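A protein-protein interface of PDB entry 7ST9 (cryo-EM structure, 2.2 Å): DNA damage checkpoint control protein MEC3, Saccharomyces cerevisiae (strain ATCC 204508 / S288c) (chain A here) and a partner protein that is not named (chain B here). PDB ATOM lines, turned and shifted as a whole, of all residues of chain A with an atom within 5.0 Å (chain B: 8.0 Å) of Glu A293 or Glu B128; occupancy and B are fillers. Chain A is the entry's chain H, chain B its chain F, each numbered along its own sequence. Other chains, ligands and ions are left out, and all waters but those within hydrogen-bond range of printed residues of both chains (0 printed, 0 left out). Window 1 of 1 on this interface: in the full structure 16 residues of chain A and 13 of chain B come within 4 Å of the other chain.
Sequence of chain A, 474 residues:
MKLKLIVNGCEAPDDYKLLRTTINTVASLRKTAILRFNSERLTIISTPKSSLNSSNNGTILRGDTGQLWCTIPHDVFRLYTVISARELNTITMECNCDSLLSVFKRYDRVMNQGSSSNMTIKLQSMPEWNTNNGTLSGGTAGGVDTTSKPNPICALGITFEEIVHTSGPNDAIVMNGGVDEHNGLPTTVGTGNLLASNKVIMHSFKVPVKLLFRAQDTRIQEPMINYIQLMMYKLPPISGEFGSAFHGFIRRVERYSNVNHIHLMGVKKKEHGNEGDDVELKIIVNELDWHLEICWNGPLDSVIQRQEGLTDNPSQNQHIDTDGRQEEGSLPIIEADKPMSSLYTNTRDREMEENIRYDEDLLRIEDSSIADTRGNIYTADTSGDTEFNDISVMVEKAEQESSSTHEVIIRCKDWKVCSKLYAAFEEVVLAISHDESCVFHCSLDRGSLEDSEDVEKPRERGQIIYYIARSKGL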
ATOM      1  N   ARG A 252       7.944  17.714 -14.311  1.00  0.00           N
ATOM      2  CA  ARG A 252       7.863  18.920 -13.493  1.00  0.00           C
ATOM      3  C   ARG A 252       6.847  18.757 -12.367  1.00  0.00           C
ATOM      4  O   ARG A 252       7.122  19.099 -11.211  1.00  0.00           O
ATOM      5  CB  ARG A 252       7.507  20.120 -14.372  1.00  0.00           C
ATOM      6  CG  ARG A 252       7.455  21.454 -13.636  1.00  0.00           C
ATOM      7  CD  ARG A 252       8.778  21.794 -12.965  1.00  0.00           C
ATOM      8  NE  ARG A 252       9.871  21.894 -13.925  1.00  0.00           N
ATOM      9  CZ  ARG A 252      10.010  22.877 -14.805  1.00  0.00           C
ATOM     10  NH1 ARG A 252       9.139  23.871 -14.876  1.00  0.00           N
ATOM     11  NH2 ARG A 252      11.049  22.862 -15.635  1.00  0.00           N
ATOM     12  N   TYR A 256       5.640  18.533  -6.832  1.00  0.00           N
ATOM     13  CA  TYR A 256       4.570  18.781  -5.871  1.00  0.00           C
ATOM     14  C   TYR A 256       4.100  17.437  -5.325  1.00  0.00           C
ATOM     15  O   TYR A 256       3.434  16.673  -6.031  1.00  0.00           O
ATOM     16  CB  TYR A 256       3.422  19.548  -6.523  1.00  0.00           C
ATOM     17  CG  TYR A 256       3.868  20.798  -7.248  1.00  0.00           C
ATOM     18  CD1 TYR A 256       4.274  20.747  -8.575  1.00  0.00           C
ATOM     19  CD2 TYR A 256       3.890  22.028  -6.604  1.00  0.00           C
ATOM     20  CE1 TYR A 256       4.685  21.886  -9.240  1.00  0.00           C
ATOM     21  CE2 TYR A 256       4.300  23.172  -7.261  1.00  0.00           C
ATOM     22  CZ  TYR A 256       4.697  23.095  -8.579  1.00  0.00           C
ATOM     23  OH  TYR A 256       5.104  24.231  -9.238  1.00  0.00           O
ATOM     24  N   LYS A 282      -0.344  21.848 -22.404  1.00  0.00           N
ATOM     25  CA  LYS A 282      -0.292  22.455 -21.082  1.00  0.00           C
ATOM     26  C   LYS A 282      -0.689  21.433 -20.028  1.00  0.00           C
ATOM     27  O   LYS A 282      -1.503  20.540 -20.277  1.00  0.00           O
ATOM     28  CB  LYS A 282      -1.220  23.674 -20.990  1.00  0.00           C
ATOM     29  CG  LYS A 282      -0.758  24.870 -21.810  1.00  0.00           C
ATOM     30  CD  LYS A 282      -1.557  26.136 -21.500  1.00  0.00           C
ATOM     31  CE  LYS A 282      -3.021  25.849 -21.201  1.00  0.00           C
ATOM     32  NZ  LYS A 282      -3.841  27.092 -21.206  1.00  0.00           N
ATOM     33  N   ILE A 283      -0.106  21.582 -18.841  1.00  0.00           N
ATOM     34  CA  ILE A 283      -0.445  20.774 -17.674  1.00  0.00           C
ATOM     35  C   ILE A 283      -0.948  21.717 -16.591  1.00  0.00           C
ATOM     36  O   ILE A 283      -0.244  22.656 -16.201  1.00  0.00           O
ATOM     37  CB  ILE A 283       0.757  19.954 -17.175  1.00  0.00           C
ATOM     38  CG1 ILE A 283       1.308  19.081 -18.305  1.00  0.00           C
ATOM     39  CG2 ILE A 283       0.355  19.097 -15.980  1.00  0.00           C
ATOM     40  CD1 ILE A 283       2.572  18.330 -17.943  1.00  0.00           C
ATOM     41  N   ILE A 284      -2.154  21.464 -16.096  1.00  0.00           N
ATOM     42  CA  ILE A 284      -2.807  22.332 -15.126  1.00  0.00           C
ATOM     43  C   ILE A 284      -2.984  21.566 -13.824  1.00  0.00           C
ATOM     44  O   ILE A 284      -3.357  20.385 -13.826  1.00  0.00           O
ATOM     45  CB  ILE A 284      -4.162  22.850 -15.650  1.00  0.00           C
ATOM     46  CG1 ILE A 284      -3.959  23.640 -16.946  1.00  0.00           C
ATOM     47  CG2 ILE A 284      -4.847  23.711 -14.599  1.00  0.00           C
ATOM     48  CD1 ILE A 284      -5.230  23.864 -17.733  1.00  0.00           C
ATOM     49  N   HIS A 291      -3.562  28.404  -8.202  1.00  0.00           N
ATOM     50  CA  HIS A 291      -3.691  27.785  -9.515  1.00  0.00           C
ATOM     51  C   HIS A 291      -2.324  27.685 -10.180  1.00  0.00           C
ATOM     52  O   HIS A 291      -1.545  28.642 -10.163  1.00  0.00           O
ATOM     53  CB  HIS A 291      -4.652  28.600 -10.381  1.00  0.00           C
ATOM     54  CG  HIS A 291      -5.056  27.917 -11.649  1.00  0.00           C
ATOM     55  ND1 HIS A 291      -6.103  27.022 -11.712  1.00  0.00           N
ATOM     56  CD2 HIS A 291      -4.562  28.006 -12.907  1.00  0.00           C
ATOM     57  CE1 HIS A 291      -6.233  26.585 -12.951  1.00  0.00           C
ATOM     58  NE2 HIS A 291      -5.310  27.167 -13.696  1.00  0.00           N
ATOM     59  N   LEU A 292      -2.029  26.524 -10.765  1.00  0.00           N
ATOM     60  CA  LEU A 292      -0.733  26.281 -11.389  1.00  0.00           C
ATOM     61  C   LEU A 292      -0.927  25.845 -12.832  1.00  0.00           C
ATOM     62  O   LEU A 292      -1.726  24.945 -13.111  1.00  0.00           O
ATOM     63  CB  LEU A 292       0.060  25.222 -10.617  1.00  0.00           C
ATOM     64  CG  LEU A 292       1.403  24.805 -11.224  1.00  0.00           C
ATOM     65  CD1 LEU A 292       2.352  25.990 -11.317  1.00  0.00           C
ATOM     66  CD2 LEU A 292       2.027  23.685 -10.412  1.00  0.00           C
ATOM     67  N   GLU A 293      -0.189  26.477 -13.743  1.00  0.00           N
ATOM     68  CA  GLU A 293      -0.217  26.146 -15.162  1.00  0.00           C
ATOM     69  C   GLU A 293       1.213  26.022 -15.661  1.00  0.00           C
ATOM     70  O   GLU A 293       2.041  26.902 -15.404  1.00  0.00           O
ATOM     71  CB  GLU A 293      -0.965  27.214 -15.970  1.00  0.00           C
ATOM     72  CG  GLU A 293      -2.263  27.696 -15.334  1.00  0.00           C
ATOM     73  CD  GLU A 293      -3.415  27.754 -16.317  1.00  0.00           C
ATOM     74  OE1 GLU A 293      -3.584  28.802 -16.975  1.00  0.00           O
ATOM     75  OE2 GLU A 293      -4.159  26.757 -16.424  1.00  0.00           O
ATOM     76  N   ILE A 294       1.503  24.934 -16.372  1.00  0.00           N
ATOM     77  CA  ILE A 294       2.812  24.692 -16.967  1.00  0.00           C
ATOM     78  C   ILE A 294       2.617  24.572 -18.470  1.00  0.00           C
ATOM     79  O   ILE A 294       1.792  23.775 -18.931  1.00  0.00           O
ATOM     80  CB  ILE A 294       3.475  23.423 -16.398  1.00  0.00           C
ATOM     81  CG1 ILE A 294       3.412  23.410 -14.866  1.00  0.00           C
ATOM     82  CG2 ILE A 294       4.924  23.334 -16.851  1.00  0.00           C
ATOM     83  CD1 ILE A 294       3.589  22.033 -14.265  1.00  0.00           C
ATOM     84  N   CYS A 295       3.375  25.357 -19.229  1.00  0.00           N
ATOM     85  CA  CYS A 295       3.227  25.438 -20.675  1.00  0.00           C
ATOM     86  C   CYS A 295       4.532  25.054 -21.356  1.00  0.00           C
ATOM     87  O   CYS A 295       5.617  25.441 -20.910  1.00  0.00           O
ATOM     88  CB  CYS A 295       2.816  26.849 -21.107  1.00  0.00           C
ATOM     89  SG  CYS A 295       1.398  27.517 -20.209  1.00  0.00           S
ATOM     90  N   SER B  92       5.178  28.877  -3.566  1.00  0.00           N
ATOM     91  CA  SER B  92       5.184  28.824  -5.023  1.00  0.00           C
ATOM     92  C   SER B  92       6.564  29.156  -5.571  1.00  0.00           C
ATOM     93  O   SER B  92       7.070  28.475  -6.469  1.00  0.00           O
ATOM     94  CB  SER B  92       4.136  29.785  -5.585  1.00  0.00           C
ATOM     95  OG  SER B  92       2.894  29.638  -4.921  1.00  0.00           O
ATOM     96  N   VAL B  95       9.217  26.241  -4.756  1.00  0.00           N
ATOM     97  CA  VAL B  95       9.169  25.119  -5.693  1.00  0.00           C
ATOM     98  C   VAL B  95       9.582  25.562  -7.094  1.00  0.00           C
ATOM     99  O   VAL B  95      10.351  24.873  -7.773  1.00  0.00           O
ATOM    100  CB  VAL B  95       7.782  24.446  -5.702  1.00  0.00           C
ATOM    101  CG1 VAL B  95       7.898  23.034  -6.243  1.00  0.00           C
ATOM    102  CG2 VAL B  95       7.211  24.355  -4.307  1.00  0.00           C
ATOM    103  N   MET B  96       9.092  26.717  -7.548  1.00  0.00           N
ATOM    104  CA  MET B  96       9.375  27.140  -8.916  1.00  0.00           C
ATOM    105  C   MET B  96      10.823  27.583  -9.090  1.00  0.00           C
ATOM    106  O   MET B  96      11.340  27.565 -10.212  1.00  0.00           O
ATOM    107  CB  MET B  96       8.434  28.272  -9.325  1.00  0.00           C
ATOM    108  CG  MET B  96       7.014  27.821  -9.618  1.00  0.00           C
ATOM    109  SD  MET B  96       5.832  29.181  -9.607  1.00  0.00           S
ATOM    110  CE  MET B  96       6.573  30.277 -10.814  1.00  0.00           C
ATOM    111  N   ASN B  97      11.492  27.980  -8.006  1.00  0.00           N
ATOM    112  CA  ASN B  97      12.861  28.477  -8.073  1.00  0.00           C
ATOM    113  C   ASN B  97      13.889  27.404  -7.733  1.00  0.00           C
ATOM    114  O   ASN B  97      15.054  27.730  -7.483  1.00  0.00           O
ATOM    115  CB  ASN B  97      13.032  29.680  -7.144  1.00  0.00           C
ATOM    116  CG  ASN B  97      14.255  30.512  -7.488  1.00  0.00           C
ATOM    117  OD1 ASN B  97      14.843  30.358  -8.558  1.00  0.00           O
ATOM    118  ND2 ASN B  97      14.644  31.399  -6.578  1.00  0.00           N
ATOM    119  N   GLU B 105      13.406  34.629 -17.260  1.00  0.00           N
ATOM    120  CA  GLU B 105      12.532  35.793 -17.214  1.00  0.00           C
ATOM    121  C   GLU B 105      11.503  35.622 -16.107  1.00  0.00           C
ATOM    122  O   GLU B 105      11.083  34.508 -15.788  1.00  0.00           O
ATOM    123  CB  GLU B 105      11.834  36.020 -18.560  1.00  0.00           C
ATOM    124  CG  GLU B 105      11.338  37.440 -18.770  1.00  0.00           C
ATOM    125  CD  GLU B 105      10.687  37.634 -20.126  1.00  0.00           C
ATOM    126  OE1 GLU B 105      11.360  37.392 -21.150  1.00  0.00           O
ATOM    127  OE2 GLU B 105       9.503  38.030 -20.168  1.00  0.00           O
ATOM    128  N   CYS B 106      11.084  36.752 -15.541  1.00  0.00           N
ATOM    129  CA  CYS B 106      10.092  36.768 -14.470  1.00  0.00           C
ATOM    130  C   CYS B 106       9.158  37.940 -14.710  1.00  0.00           C
ATOM    131  O   CYS B 106       9.622  39.079 -14.821  1.00  0.00           O
ATOM    132  CB  CYS B 106      10.767  36.892 -13.104  1.00  0.00           C
ATOM    133  SG  CYS B 106       9.946  35.997 -11.782  1.00  0.00           S
ATOM    134  N   THR B 107       7.852  37.682 -14.781  1.00  0.00           N
ATOM    135  CA  THR B 107       6.897  38.751 -15.039  1.00  0.00           C
ATOM    136  C   THR B 107       5.728  38.694 -14.065  1.00  0.00           C
ATOM    137  O   THR B 107       5.161  37.627 -13.801  1.00  0.00           O
ATOM    138  CB  THR B 107       6.375  38.712 -16.486  1.00  0.00           C
ATOM    139  OG1 THR B 107       5.423  39.765 -16.682  1.00  0.00           O
ATOM    140  CG2 THR B 107       5.721  37.389 -16.794  1.00  0.00           C
ATOM    141  N   VAL B 118      -0.805  37.563 -11.010  1.00  0.00           N
ATOM    142  CA  VAL B 118      -0.226  36.531 -11.861  1.00  0.00           C
ATOM    143  C   VAL B 118       1.291  36.647 -11.828  1.00  0.00           C
ATOM    144  O   VAL B 118       1.848  37.719 -12.093  1.00  0.00           O
ATOM    145  CB  VAL B 118      -0.755  36.640 -13.301  1.00  0.00           C
ATOM    146  CG1 VAL B 118      -0.027  35.663 -14.213  1.00  0.00           C
ATOM    147  CG2 VAL B 118      -2.256  36.394 -13.333  1.00  0.00           C
ATOM    148  N   LEU B 119       1.955  35.537 -11.510  1.00  0.00           N
ATOM    149  CA  LEU B 119       3.408  35.431 -11.500  1.00  0.00           C
ATOM    150  C   LEU B 119       3.803  34.377 -12.523  1.00  0.00           C
ATOM    151  O   LEU B 119       3.344  33.233 -12.442  1.00  0.00           O
ATOM    152  CB  LEU B 119       3.909  35.045 -10.107  1.00  0.00           C
ATOM    153  CG  LEU B 119       5.413  35.081  -9.834  1.00  0.00           C
ATOM    154  CD1 LEU B 119       5.781  36.331  -9.064  1.00  0.00           C
ATOM    155  CD2 LEU B 119       5.838  33.836  -9.069  1.00  0.00           C
ATOM    156  N   ILE B 120       4.650  34.751 -13.481  1.00  0.00           N
ATOM    157  CA  ILE B 120       5.065  33.829 -14.533  1.00  0.00           C
ATOM    158  C   ILE B 120       6.585  33.766 -14.558  1.00  0.00           C
ATOM    159  O   ILE B 120       7.255  34.799 -14.689  1.00  0.00           O
ATOM    160  CB  ILE B 120       4.514  34.235 -15.909  1.00  0.00           C
ATOM    161  CG1 ILE B 120       2.986  34.143 -15.917  1.00  0.00           C
ATOM    162  CG2 ILE B 120       5.110  33.358 -17.002  1.00  0.00           C
ATOM    163  CD1 ILE B 120       2.334  34.851 -17.089  1.00  0.00           C
ATOM    164  N   PHE B 121       7.120  32.552 -14.431  1.00  0.00           N
ATOM    165  CA  PHE B 121       8.538  32.273 -14.612  1.00  0.00           C
ATOM    166  C   PHE B 121       8.721  31.682 -16.004  1.00  0.00           C
ATOM    167  O   PHE B 121       8.207  30.596 -16.289  1.00  0.00           O
ATOM    168  CB  PHE B 121       9.047  31.289 -13.558  1.00  0.00           C
ATOM    169  CG  PHE B 121       9.374  31.920 -12.235  1.00  0.00           C
ATOM    170  CD1 PHE B 121       8.502  32.813 -11.638  1.00  0.00           C
ATOM    171  CD2 PHE B 121      10.554  31.607 -11.581  1.00  0.00           C
ATOM    172  CE1 PHE B 121       8.802  33.382 -10.417  1.00  0.00           C
ATOM    173  CE2 PHE B 121      10.861  32.177 -10.361  1.00  0.00           C
ATOM    174  CZ  PHE B 121       9.984  33.067  -9.780  1.00  0.00           C
ATOM    175  N   GLU B 122       9.452  32.385 -16.863  1.00  0.00           N
ATOM    176  CA  GLU B 122       9.658  31.966 -18.244  1.00  0.00           C
ATOM    177  C   GLU B 122      11.078  31.441 -18.400  1.00  0.00           C
ATOM    178  O   GLU B 122      12.048  32.158 -18.121  1.00  0.00           O
ATOM    179  CB  GLU B 122       9.399  33.121 -19.211  1.00  0.00           C
ATOM    180  CG  GLU B 122       8.001  33.130 -19.814  1.00  0.00           C
ATOM    181  CD  GLU B 122       8.006  33.440 -21.299  1.00  0.00           C
ATOM    182  OE1 GLU B 122       8.869  34.228 -21.742  1.00  0.00           O
ATOM    183  OE2 GLU B 122       7.147  32.896 -22.024  1.00  0.00           O
ATOM    184  N   ASP B 123      11.188  30.189 -18.840  1.00  0.00           N
ATOM    185  CA  ASP B 123      12.447  29.524 -19.119  1.00  0.00           C
ATOM    186  C   ASP B 123      12.673  29.484 -20.630  1.00  0.00           C
ATOM    187  O   ASP B 123      11.934  30.095 -21.409  1.00  0.00           O
ATOM    188  CB  ASP B 123      12.439  28.124 -18.500  1.00  0.00           C
ATOM    189  CG  ASP B 123      13.834  27.599 -18.221  1.00  0.00           C
ATOM    190  OD1 ASP B 123      14.806  28.195 -18.729  1.00  0.00           O
ATOM    191  OD2 ASP B 123      13.957  26.592 -17.493  1.00  0.00           O
ATOM    192  N   PHE B 125      12.265  26.980 -22.729  1.00  0.00           N
ATOM    193  CA  PHE B 125      11.183  26.284 -23.409  1.00  0.00           C
ATOM    194  C   PHE B 125       9.995  25.963 -22.511  1.00  0.00           C
ATOM    195  O   PHE B 125       8.996  25.432 -23.009  1.00  0.00           O
ATOM    196  CB  PHE B 125      11.697  24.975 -24.031  1.00  0.00           C
ATOM    197  CG  PHE B 125      12.771  25.174 -25.062  1.00  0.00           C
ATOM    198  CD1 PHE B 125      12.491  25.808 -26.261  1.00  0.00           C
ATOM    199  CD2 PHE B 125      14.061  24.723 -24.834  1.00  0.00           C
ATOM    200  CE1 PHE B 125      13.476  25.991 -27.212  1.00  0.00           C
ATOM    201  CE2 PHE B 125      15.050  24.904 -25.781  1.00  0.00           C
ATOM    202  CZ  PHE B 125      14.758  25.539 -26.971  1.00  0.00           C
ATOM    203  N   ILE B 126      10.067  26.261 -21.215  1.00  0.00           N
ATOM    204  CA  ILE B 126       8.999  25.951 -20.272  1.00  0.00           C
ATOM    205  C   ILE B 126       8.662  27.210 -19.490  1.00  0.00           C
ATOM    206  O   ILE B 126       9.560  27.884 -18.972  1.00  0.00           O
ATOM    207  CB  ILE B 126       9.394  24.810 -19.314  1.00  0.00           C
ATOM    208  CG1 ILE B 126       9.680  23.527 -20.097  1.00  0.00           C
ATOM    209  CG2 ILE B 126       8.291  24.572 -18.291  1.00  0.00           C
ATOM    210  CD1 ILE B 126      10.457  22.490 -19.311  1.00  0.00           C
ATOM    211  N   SER B 127       7.371  27.524 -19.400  1.00  0.00           N
ATOM    212  CA  SER B 127       6.882  28.668 -18.642  1.00  0.00           C
ATOM    213  C   SER B 127       5.891  28.183 -17.594  1.00  0.00           C
ATOM    214  O   SER B 127       4.996  27.389 -17.900  1.00  0.00           O
ATOM    215  CB  SER B 127       6.221  29.701 -19.558  1.00  0.00           C
ATOM    216  OG  SER B 127       4.950  29.254 -19.995  1.00  0.00           O
ATOM    217  N   GLU B 128       6.054  28.663 -16.364  1.00  0.00           N
ATOM    218  CA  GLU B 128       5.199  28.294 -15.242  1.00  0.00           C
ATOM    219  C   GLU B 128       4.422  29.524 -14.795  1.00  0.00           C
ATOM    220  O   GLU B 128       5.019  30.558 -14.476  1.00  0.00           O
ATOM    221  CB  GLU B 128       6.029  27.730 -14.090  1.00  0.00           C
ATOM    222  CG  GLU B 128       5.391  26.550 -13.374  1.00  0.00           C
ATOM    223  CD  GLU B 128       6.417  25.572 -12.834  1.00  0.00           C
ATOM    224  OE1 GLU B 128       7.263  25.101 -13.624  1.00  0.00           O
ATOM    225  OE2 GLU B 128       6.378  25.271 -11.622  1.00  0.00           O
ATOM    226  N   ARG B 129       3.096  29.409 -14.762  1.00  0.00           N
ATOM    227  CA  ARG B 129       2.206  30.513 -14.431  1.00  0.00           C
ATOM    228  C   ARG B 129       1.417  30.156 -13.180  1.00  0.00           C
ATOM    229  O   ARG B 129       0.784  29.097 -13.123  1.00  0.00           O
ATOM    230  CB  ARG B 129       1.260  30.811 -15.600  1.00  0.00           C
ATOM    231  CG  ARG B 129       0.176  31.846 -15.315  1.00  0.00           C
ATOM    232  CD  ARG B 129      -0.942  31.755 -16.341  1.00  0.00           C
ATOM    233  NE  ARG B 129      -2.062  32.634 -16.021  1.00  0.00           N
ATOM    234  CZ  ARG B 129      -2.219  33.863 -16.492  1.00  0.00           C
ATOM    235  NH1 ARG B 129      -1.337  34.411 -17.313  1.00  0.00           N
ATOM    236  NH2 ARG B 129      -3.291  34.564 -16.130  1.00  0.00           N
ATOM    237  N   VAL B 130       1.449  31.041 -12.184  1.00  0.00           N
ATOM    238  CA  VAL B 130       0.723  30.846 -10.935  1.00  0.00           C
ATOM    239  C   VAL B 130      -0.123  32.081 -10.663  1.00  0.00           C
ATOM    240  O   VAL B 130       0.333  33.216 -10.845  1.00  0.00           O
ATOM    241  CB  VAL B 130       1.674  30.562  -9.753  1.00  0.00           C
ATOM    242  CG1 VAL B 130       2.467  29.292 -10.007  1.00  0.00           C
ATOM    243  CG2 VAL B 130       2.607  31.734  -9.517  1.00  0.00           C
ATOM    244  N   GLU B 131      -1.361  31.856 -10.233  1.00  0.00           N
ATOM    245  CA  GLU B 131      -2.304  32.924  -9.930  1.00  0.00           C
ATOM    246  C   GLU B 131      -2.579  32.921  -8.432  1.00  0.00           C
ATOM    247  O   GLU B 131      -2.983  31.896  -7.874  1.00  0.00           O
ATOM    248  CB  GLU B 131      -3.601  32.741 -10.716  1.00  0.00           C
ATOM    249  CG  GLU B 131      -3.396  32.561 -12.210  1.00  0.00           C
ATOM    250  CD  GLU B 131      -4.699  32.580 -12.981  1.00  0.00           C
ATOM    251  OE1 GLU B 131      -5.749  32.265 -12.383  1.00  0.00           O
ATOM    252  OE2 GLU B 131      -4.675  32.909 -14.186  1.00  0.00           O
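The backbone NH (N) of Cys A295 sits at hydrogen-bond distance from the backbone carbonyl oxygen (O) of Ser B127 (2.9 Å). OE1 of Glu B128 is in salt-bridge range of NH1 of Arg A252, 2.6 Å away. OH of Tyr A256 sits at hydrogen-bond distance from OE2 of Glu B128 (2.9 Å). The backbone carbonyl oxygen (O) of Glu A293 sits at hydrogen-bond distance from the backbone NH (N) of Arg B129 (2.8 Å). N of Glu B131 is in hydrogen-bond range of O of His A291 (3.2 Å).
The backbone carbonyl oxygen (O) of Val B130 sits at hydrogen-bond distance from the backbone NH (N) of Leu B119, 2.9 Å away. The backbone NH (N) of Glu B128 sits at hydrogen-bond distance from the backbone carbonyl oxygen (O) of Phe B121 (2.9 Å). The side-chain carboxylate (OE2) of Glu B131 is in salt-bridge range of the guanidinium group (NH2) of Arg B129, 2.9 Å away. The backbone NH (N) of Ile A294 lies within hydrogen-bond range of the backbone carbonyl oxygen (O) of Ile A283 (2.9 Å). A ring nitrogen (NE2) of His A291 is in hydrogen-bond range of the side-chain carboxylate (OE2) of Glu A293, at 3.0 Å.
Among the printed residues, pairs that only touch across the chains: His A291 with Val B130, Glu A293 with Glu B128, Cys A295 with Ile B126, Leu A292 with Val B130, Arg A252 with Ile B126, Ile A294 with Ser B127, Leu A292 with Arg B129, Leu A292 with Glu B128, Tyr A256 with Val B95, His A291 with Arg B129, Ile A294 with Ile B126, Glu A293 with Ser B127 and Cys A295 with Phe B125.
Thr B107 touches none of the printed residues of chain A. Printed residues of chain A within 4 Å of Phe B125: Cys A295 (3.98 Å). Of the printed residues of chain A, Ile B126 touches Arg A252, Ile A294 and Cys A295. Of the printed residues of chain A, Ser B127 touches Glu A293 (3.9 Å), Ile A294 (3.6 Å) and Cys A295 (2.9 Å). Of the printed residues of chain A, Glu B128 touches Arg A252 (2.6 Å), Tyr A256 (2.9 Å), Leu A292 (3.7 Å) and Glu A293 (3.5 Å). Of the printed residues of chain A, Arg B129 touches His A291, Leu A292 and Glu A293. Of the printed residues of chain A, Glu B131 touches His A291. The nearest printed residue of chain B that does not touch Cys A295 is Glu B128 (5.1 Å).
Printed residues of chain B that touch a printed residue of chain A: Val B95, Phe B125, Ile B126, Ser B127, Glu B128, Arg B129, Val B130 and Glu B131. Hydrophobic or aromatic side chains of chain B within 4 Å of the printed part of chain A: Val B95, Ile B126 and Val B130. Of the 10 printed residues of chain A, 7 touch a printed residue of chain B. Hydrophobic or aromatic side chains of chain A that line the printed part of chain B: Tyr A256, Leu A292 and Ile A294. Along chain A the printed residues that touch a printed residue of chain B span positions 252 to 295. Among the printed residues, 18 pairs touch across the chains. Among the printed residues, Asp or Glu carboxylates within 4 Å of a Lys or Arg side-chain nitrogen of the other chain: Arg A252 with Glu B128 (2.6 Å).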
